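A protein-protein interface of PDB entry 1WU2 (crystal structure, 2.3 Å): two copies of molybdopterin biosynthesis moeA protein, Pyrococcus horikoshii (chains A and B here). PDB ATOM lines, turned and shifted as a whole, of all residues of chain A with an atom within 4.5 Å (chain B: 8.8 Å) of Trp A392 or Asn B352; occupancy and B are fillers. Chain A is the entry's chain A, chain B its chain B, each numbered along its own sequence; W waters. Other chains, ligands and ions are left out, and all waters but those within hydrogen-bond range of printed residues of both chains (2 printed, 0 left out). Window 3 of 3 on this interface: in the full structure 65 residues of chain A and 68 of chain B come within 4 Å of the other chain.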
ATOM      1  N   LYS A 327     -19.632 -22.594  12.439  1.00  0.00           N
ATOM      2  CA  LYS A 327     -20.595 -22.794  11.363  1.00  0.00           C
ATOM      3  C   LYS A 327     -21.229 -24.178  11.475  1.00  0.00           C
ATOM      4  O   LYS A 327     -20.534 -25.176  11.659  1.00  0.00           O
ATOM      5  CB  LYS A 327     -19.928 -22.614  10.000  1.00  0.00           C
ATOM      6  CG  LYS A 327     -19.757 -21.154   9.591  1.00  0.00           C
ATOM      7  CD  LYS A 327     -19.897 -20.959   8.080  1.00  0.00           C
ATOM      8  CE  LYS A 327     -19.855 -19.480   7.695  1.00  0.00           C
ATOM      9  NZ  LYS A 327     -18.787 -18.731   8.428  1.00  0.00           N
ATOM     10  N   VAL A 328     -22.553 -24.217  11.353  1.00  0.00           N
ATOM     11  CA  VAL A 328     -23.345 -25.421  11.582  1.00  0.00           C
ATOM     12  C   VAL A 328     -24.257 -25.712  10.387  1.00  0.00           C
ATOM     13  O   VAL A 328     -24.862 -24.803   9.819  1.00  0.00           O
ATOM     14  CB  VAL A 328     -24.206 -25.273  12.858  1.00  0.00           C
ATOM     15  CG1 VAL A 328     -25.033 -26.525  13.111  1.00  0.00           C
ATOM     16  CG2 VAL A 328     -23.325 -24.962  14.061  1.00  0.00           C
ATOM     17  N   LYS A 329     -24.348 -26.988  10.019  1.00  0.00           N
ATOM     18  CA  LYS A 329     -25.253 -27.450   8.965  1.00  0.00           C
ATOM     19  C   LYS A 329     -26.637 -27.690   9.569  1.00  0.00           C
ATOM     20  O   LYS A 329     -26.754 -28.315  10.617  1.00  0.00           O
ATOM     21  CB  LYS A 329     -24.709 -28.745   8.351  1.00  0.00           C
ATOM     22  CG  LYS A 329     -25.550 -29.344   7.218  1.00  0.00           C
ATOM     23  CD  LYS A 329     -25.291 -30.851   7.056  1.00  0.00           C
ATOM     24  CE  LYS A 329     -24.790 -31.197   5.657  1.00  0.00           C
ATOM     25  NZ  LYS A 329     -24.252 -32.587   5.584  1.00  0.00           N
ATOM     26  N   LEU A 376     -28.186 -16.594   9.469  1.00  0.00           N
ATOM     27  CA  LEU A 376     -27.959 -17.121   8.140  1.00  0.00           C
ATOM     28  C   LEU A 376     -27.699 -15.942   7.215  1.00  0.00           C
ATOM     29  O   LEU A 376     -28.359 -14.914   7.315  1.00  0.00           O
ATOM     30  CB  LEU A 376     -29.199 -17.894   7.681  1.00  0.00           C
ATOM     31  CG  LEU A 376     -29.336 -18.189   6.188  1.00  0.00           C
ATOM     32  CD1 LEU A 376     -28.263 -19.154   5.743  1.00  0.00           C
ATOM     33  CD2 LEU A 376     -30.714 -18.741   5.897  1.00  0.00           C
ATOM     34  N   VAL A 391     -28.804 -25.459   4.968  1.00  0.00           N
ATOM     35  CA  VAL A 391     -28.164 -24.150   5.018  1.00  0.00           C
ATOM     36  C   VAL A 391     -27.063 -24.125   6.071  1.00  0.00           C
ATOM     37  O   VAL A 391     -27.066 -24.922   7.010  1.00  0.00           O
ATOM     38  CB  VAL A 391     -29.186 -23.029   5.328  1.00  0.00           C
ATOM     39  CG1 VAL A 391     -30.208 -22.920   4.209  1.00  0.00           C
ATOM     40  CG2 VAL A 391     -29.881 -23.264   6.674  1.00  0.00           C
ATOM     41  N   TRP A 392     -26.125 -23.199   5.894  1.00  0.00           N
ATOM     42  CA  TRP A 392     -25.042 -22.976   6.838  1.00  0.00           C
ATOM     43  C   TRP A 392     -25.353 -21.729   7.651  1.00  0.00           C
ATOM     44  O   TRP A 392     -25.695 -20.684   7.095  1.00  0.00           O
ATOM     45  CB  TRP A 392     -23.715 -22.825   6.094  1.00  0.00           C
ATOM     46  CG  TRP A 392     -23.379 -24.048   5.317  1.00  0.00           C
ATOM     47  CD1 TRP A 392     -23.736 -24.328   4.030  1.00  0.00           C
ATOM     48  CD2 TRP A 392     -22.653 -25.186   5.787  1.00  0.00           C
ATOM     49  NE1 TRP A 392     -23.264 -25.566   3.664  1.00  0.00           N
ATOM     50  CE2 TRP A 392     -22.595 -26.116   4.725  1.00  0.00           C
ATOM     51  CE3 TRP A 392     -22.037 -25.517   7.000  1.00  0.00           C
ATOM     52  CZ2 TRP A 392     -21.947 -27.347   4.840  1.00  0.00           C
ATOM     53  CZ3 TRP A 392     -21.395 -26.739   7.114  1.00  0.00           C
ATOM     54  CH2 TRP A 392     -21.354 -27.640   6.040  1.00  0.00           C
ATOM     55  N   ILE A 393     -25.250 -21.855   8.970  1.00  0.00           N
ATOM     56  CA  ILE A 393     -25.556 -20.765   9.885  1.00  0.00           C
ATOM     57  C   ILE A 393     -24.396 -20.543  10.846  1.00  0.00           C
ATOM     58  O   ILE A 393     -23.561 -21.423  11.034  1.00  0.00           O
ATOM     59  CB  ILE A 393     -26.872 -21.053  10.658  1.00  0.00           C
ATOM     60  CG1 ILE A 393     -26.731 -22.288  11.558  1.00  0.00           C
ATOM     61  CG2 ILE A 393     -28.022 -21.236   9.680  1.00  0.00           C
ATOM     62  CD1 ILE A 393     -27.930 -22.539  12.443  1.00  0.00           C
ATOM     63  N   VAL B 328     -24.827 -30.338  17.578  1.00  0.00           N
ATOM     64  CA  VAL B 328     -24.864 -30.160  16.127  1.00  0.00           C
ATOM     65  C   VAL B 328     -24.731 -31.489  15.375  1.00  0.00           C
ATOM     66  O   VAL B 328     -24.348 -32.502  15.950  1.00  0.00           O
ATOM     67  CB  VAL B 328     -23.769 -29.162  15.647  1.00  0.00           C
ATOM     68  CG1 VAL B 328     -23.824 -27.869  16.458  1.00  0.00           C
ATOM     69  CG2 VAL B 328     -22.377 -29.777  15.728  1.00  0.00           C
ATOM     70  N   LYS B 329     -25.058 -31.460  14.084  1.00  0.00           N
ATOM     71  CA  LYS B 329     -24.983 -32.636  13.219  1.00  0.00           C
ATOM     72  C   LYS B 329     -23.708 -32.582  12.393  1.00  0.00           C
ATOM     73  O   LYS B 329     -23.441 -31.581  11.731  1.00  0.00           O
ATOM     74  CB  LYS B 329     -26.178 -32.692  12.263  1.00  0.00           C
ATOM     75  CG  LYS B 329     -27.500 -33.089  12.907  1.00  0.00           C
ATOM     76  CD  LYS B 329     -28.580 -33.335  11.846  1.00  0.00           C
ATOM     77  CE  LYS B 329     -29.505 -34.489  12.218  1.00  0.00           C
ATOM     78  NZ  LYS B 329     -30.783 -34.439  11.445  1.00  0.00           N
ATOM     79  N   ALA B 330     -22.931 -33.660  12.429  1.00  0.00           N
ATOM     80  CA  ALA B 330     -21.705 -33.764  11.641  1.00  0.00           C
ATOM     81  C   ALA B 330     -21.562 -35.148  11.004  1.00  0.00           C
ATOM     82  O   ALA B 330     -22.249 -36.095  11.386  1.00  0.00           O
ATOM     83  CB  ALA B 330     -20.502 -33.456  12.512  1.00  0.00           C
ATOM     84  N   ILE B 331     -20.655 -35.247  10.035  1.00  0.00           N
ATOM     85  CA  ILE B 331     -20.388 -36.490   9.318  1.00  0.00           C
ATOM     86  C   ILE B 331     -19.017 -37.014   9.731  1.00  0.00           C
ATOM     87  O   ILE B 331     -18.028 -36.301   9.628  1.00  0.00           O
ATOM     88  CB  ILE B 331     -20.421 -36.251   7.785  1.00  0.00           C
ATOM     89  CG1 ILE B 331     -21.778 -35.688   7.341  1.00  0.00           C
ATOM     90  CG2 ILE B 331     -20.094 -37.539   7.024  1.00  0.00           C
ATOM     91  CD1 ILE B 331     -22.955 -36.646   7.505  1.00  0.00           C
ATOM     92  N   TYR B 349     -12.729 -33.145  16.591  1.00  0.00           N
ATOM     93  CA  TYR B 349     -12.607 -31.790  16.060  1.00  0.00           C
ATOM     94  C   TYR B 349     -13.681 -31.539  15.003  1.00  0.00           C
ATOM     95  O   TYR B 349     -13.651 -32.142  13.930  1.00  0.00           O
ATOM     96  CB  TYR B 349     -11.219 -31.564  15.456  1.00  0.00           C
ATOM     97  CG  TYR B 349     -10.952 -30.119  15.118  1.00  0.00           C
ATOM     98  CD1 TYR B 349     -10.476 -29.237  16.083  1.00  0.00           C
ATOM     99  CD2 TYR B 349     -11.188 -29.627  13.838  1.00  0.00           C
ATOM    100  CE1 TYR B 349     -10.232 -27.901  15.781  1.00  0.00           C
ATOM    101  CE2 TYR B 349     -10.949 -28.292  13.526  1.00  0.00           C
ATOM    102  CZ  TYR B 349     -10.472 -27.436  14.504  1.00  0.00           C
ATOM    103  OH  TYR B 349     -10.231 -26.116  14.213  1.00  0.00           O
ATOM    104  N   TYR B 350     -14.628 -30.657  15.318  1.00  0.00           N
ATOM    105  CA  TYR B 350     -15.709 -30.293  14.404  1.00  0.00           C
ATOM    106  C   TYR B 350     -15.361 -29.038  13.597  1.00  0.00           C
ATOM    107  O   TYR B 350     -14.812 -28.077  14.138  1.00  0.00           O
ATOM    108  CB  TYR B 350     -17.013 -30.059  15.176  1.00  0.00           C
ATOM    109  CG  TYR B 350     -18.098 -29.448  14.322  1.00  0.00           C
ATOM    110  CD1 TYR B 350     -18.366 -28.086  14.377  1.00  0.00           C
ATOM    111  CD2 TYR B 350     -18.826 -30.226  13.430  1.00  0.00           C
ATOM    112  CE1 TYR B 350     -19.341 -27.516  13.584  1.00  0.00           C
ATOM    113  CE2 TYR B 350     -19.808 -29.666  12.631  1.00  0.00           C
ATOM    114  CZ  TYR B 350     -20.059 -28.308  12.713  1.00  0.00           C
ATOM    115  OH  TYR B 350     -21.029 -27.738  11.922  1.00  0.00           O
ATOM    116  N   GLU B 351     -15.704 -29.052  12.310  1.00  0.00           N
ATOM    117  CA  GLU B 351     -15.462 -27.920  11.414  1.00  0.00           C
ATOM    118  C   GLU B 351     -16.268 -28.064  10.121  1.00  0.00           C
ATOM    119  O   GLU B 351     -16.060 -29.012   9.361  1.00  0.00           O
ATOM    120  CB  GLU B 351     -13.974 -27.815  11.074  1.00  0.00           C
ATOM    121  CG  GLU B 351     -13.589 -26.529  10.359  1.00  0.00           C
ATOM    122  CD  GLU B 351     -12.141 -26.525   9.917  1.00  0.00           C
ATOM    123  OE1 GLU B 351     -11.743 -27.451   9.174  1.00  0.00           O
ATOM    124  OE2 GLU B 351     -11.400 -25.600  10.317  1.00  0.00           O
ATOM    125  N   ASN B 352     -17.179 -27.119   9.881  1.00  0.00           N
ATOM    126  CA  ASN B 352     -17.999 -27.083   8.666  1.00  0.00           C
ATOM    127  C   ASN B 352     -18.632 -28.432   8.312  1.00  0.00           C
ATOM    128  O   ASN B 352     -18.429 -28.967   7.220  1.00  0.00           O
ATOM    129  CB  ASN B 352     -17.187 -26.543   7.481  1.00  0.00           C
ATOM    130  CG  ASN B 352     -16.724 -25.102   7.686  1.00  0.00           C
ATOM    131  OD1 ASN B 352     -15.685 -24.693   7.165  1.00  0.00           O
ATOM    132  ND2 ASN B 352     -17.498 -24.330   8.439  1.00  0.00           N
ATOM    133  N   GLY B 353     -19.394 -28.972   9.259  1.00  0.00           N
ATOM    134  CA  GLY B 353     -20.180 -30.175   9.046  1.00  0.00           C
ATOM    135  C   GLY B 353     -19.418 -31.490   9.052  1.00  0.00           C
ATOM    136  O   GLY B 353     -19.992 -32.521   8.711  1.00  0.00           O
ATOM    137  N   ILE B 354     -18.145 -31.464   9.441  1.00  0.00           N
ATOM    138  CA  ILE B 354     -17.296 -32.658   9.445  1.00  0.00           C
ATOM    139  C   ILE B 354     -16.803 -32.956  10.862  1.00  0.00           C
ATOM    140  O   ILE B 354     -16.302 -32.068  11.543  1.00  0.00           O
ATOM    141  CB  ILE B 354     -16.081 -32.465   8.506  1.00  0.00           C
ATOM    142  CG1 ILE B 354     -16.524 -32.037   7.097  1.00  0.00           C
ATOM    143  CG2 ILE B 354     -15.244 -33.742   8.437  1.00  0.00           C
ATOM    144  CD1 ILE B 354     -17.316 -33.084   6.329  1.00  0.00           C
ATOM    145  N   ALA B 355     -16.935 -34.207  11.292  1.00  0.00           N
ATOM    146  CA  ALA B 355     -16.451 -34.641  12.601  1.00  0.00           C
ATOM    147  C   ALA B 355     -15.227 -35.542  12.469  1.00  0.00           C
ATOM    148  O   ALA B 355     -15.357 -36.731  12.203  1.00  0.00           O
ATOM    149  CB  ALA B 355     -17.555 -35.366  13.356  1.00  0.00           C
ATOM    150  N   ASN B 373     -12.476 -29.893  19.890  1.00  0.00           N
ATOM    151  CA  ASN B 373     -13.417 -28.837  20.265  1.00  0.00           C
ATOM    152  C   ASN B 373     -14.854 -29.349  20.408  1.00  0.00           C
ATOM    153  O   ASN B 373     -15.804 -28.569  20.350  1.00  0.00           O
ATOM    154  CB  ASN B 373     -13.362 -27.689  19.247  1.00  0.00           C
ATOM    155  CG  ASN B 373     -13.847 -28.099  17.864  1.00  0.00           C
ATOM    156  OD1 ASN B 373     -14.348 -29.208  17.672  1.00  0.00           O
ATOM    157  ND2 ASN B 373     -13.701 -27.202  16.896  1.00  0.00           N
ATOM    158  N   ILE B 393     -23.069 -34.460  18.010  1.00  0.00           N
ATOM    159  CA  ILE B 393     -21.935 -34.128  18.873  1.00  0.00           C
ATOM    160  C   ILE B 393     -22.254 -32.911  19.741  1.00  0.00           C
ATOM    161  O   ILE B 393     -23.127 -32.118  19.406  1.00  0.00           O
ATOM    162  CB  ILE B 393     -20.663 -33.874  18.025  1.00  0.00           C
ATOM    163  CG1 ILE B 393     -20.858 -32.679  17.085  1.00  0.00           C
ATOM    164  CG2 ILE B 393     -20.298 -35.121  17.225  1.00  0.00           C
ATOM    165  CD1 ILE B 393     -19.581 -32.160  16.486  1.00  0.00           C
ATOM    166  N   LEU B 395     -20.596 -29.512  21.375  1.00  0.00           N
ATOM    167  CA  LEU B 395     -19.468 -28.588  21.345  1.00  0.00           C
ATOM    168  C   LEU B 395     -18.979 -28.293  22.757  1.00  0.00           C
ATOM    169  O   LEU B 395     -19.774 -28.212  23.693  1.00  0.00           O
ATOM    170  CB  LEU B 395     -19.856 -27.277  20.659  1.00  0.00           C
ATOM    171  CG  LEU B 395     -20.301 -27.367  19.198  1.00  0.00           C
ATOM    172  CD1 LEU B 395     -20.632 -25.983  18.688  1.00  0.00           C
ATOM    173  CD2 LEU B 395     -19.240 -28.022  18.325  1.00  0.00           C
HETATM  174  O   HOH W   1     -17.025 -24.460  11.930  1.00  0.00           O
HETATM  175  O   HOH W   2     -27.055 -29.595  12.701  1.00  0.00           O
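OH of Tyr B350 sits at hydrogen-bond distance from O of Lys A327, at 2.6 Å.
Of the 7 printed residues of chain A, 4 touch a printed residue of chain B.
Printed residues of chain A that touch a printed residue of chain B: Lys A327, Val A328, Lys A329 and Trp A392.
Of the 14 printed residues of chain B, 4 touch a printed residue of chain A.
Hydrophobic or aromatic side chains of chain B that line the printed part of chain A: Val B328 and Tyr B350.
Among the printed residues, 7 pairs touch across the chains.
Among the printed residues, no Asp or Glu carboxylate lies within 4 Å of a Lys or Arg side-chain nitrogen of the other chain.
Val B328 touches its own counterpart, Val A328.
Of the 7 pairs that touch across the chains among the printed residues, 1 has its exchanged pair printed and touching as well.
Printed residues of chain B within 4 Å of Val A328: Val B328 and Tyr B350.
Of the printed residues of chain B, Lys A329 touches Tyr B350.
No residue of chain B comes within 4 Å of Val A391.
Trp A392 touches two residues of chain B.
Of the printed residues of chain A, Val B328 touches Val A328.
Printed residues of chain A within 4 Å of Tyr B350: Lys A327 (2.6 Å), Val A328 (3.3 Å) and Lys A329 (3.9 Å).
Asn B352 touches two residues of chain A.
Of the printed residues of chain A, Gly B353 touches Trp A392 (3.7 Å).
The nearest residue of chain B that does not touch Trp A392 is Tyr B350 (4.9 Å).
The nearest printed residue of chain A that does not touch Asn B352 is Val A328 (5.8 Å).
Water W2 lies within hydrogen-bond range of O of Lys A329 (2.5 Å) and N of Lys B329 (3.1 Å).
Water W1 lies within hydrogen-bond range of N of Lys A327 (3.2 Å) and N of Asn B352 (3.4 Å).
Among the printed residues, pairs that only touch across the chains: Val A328 with Tyr B350, Lys A327 with Asn B352, Trp A392 with Asn B352, Trp A392 with Gly B353, Val A328 with Val B328 and Lys A329 with Tyr B350.
O of Ile A393 lies within hydrogen-bond range of N of Val A328 (3.0 Å).
N of Val B328 lies within hydrogen-bond range of O of Ile B393, 3.1 Å away.
N of Ile B331 is in hydrogen-bond range of O of Gly B353 (3.1 Å).
The side-chain hydroxyl (OH) of Tyr B350 is in hydrogen-bond range of the backbone NH (N) of Gly B353 (3.4 Å).
The side-chain amide oxygen of Asn B373 sits at hydrogen-bond distance from the backbone NH of Tyr B350 (2.8 Å).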
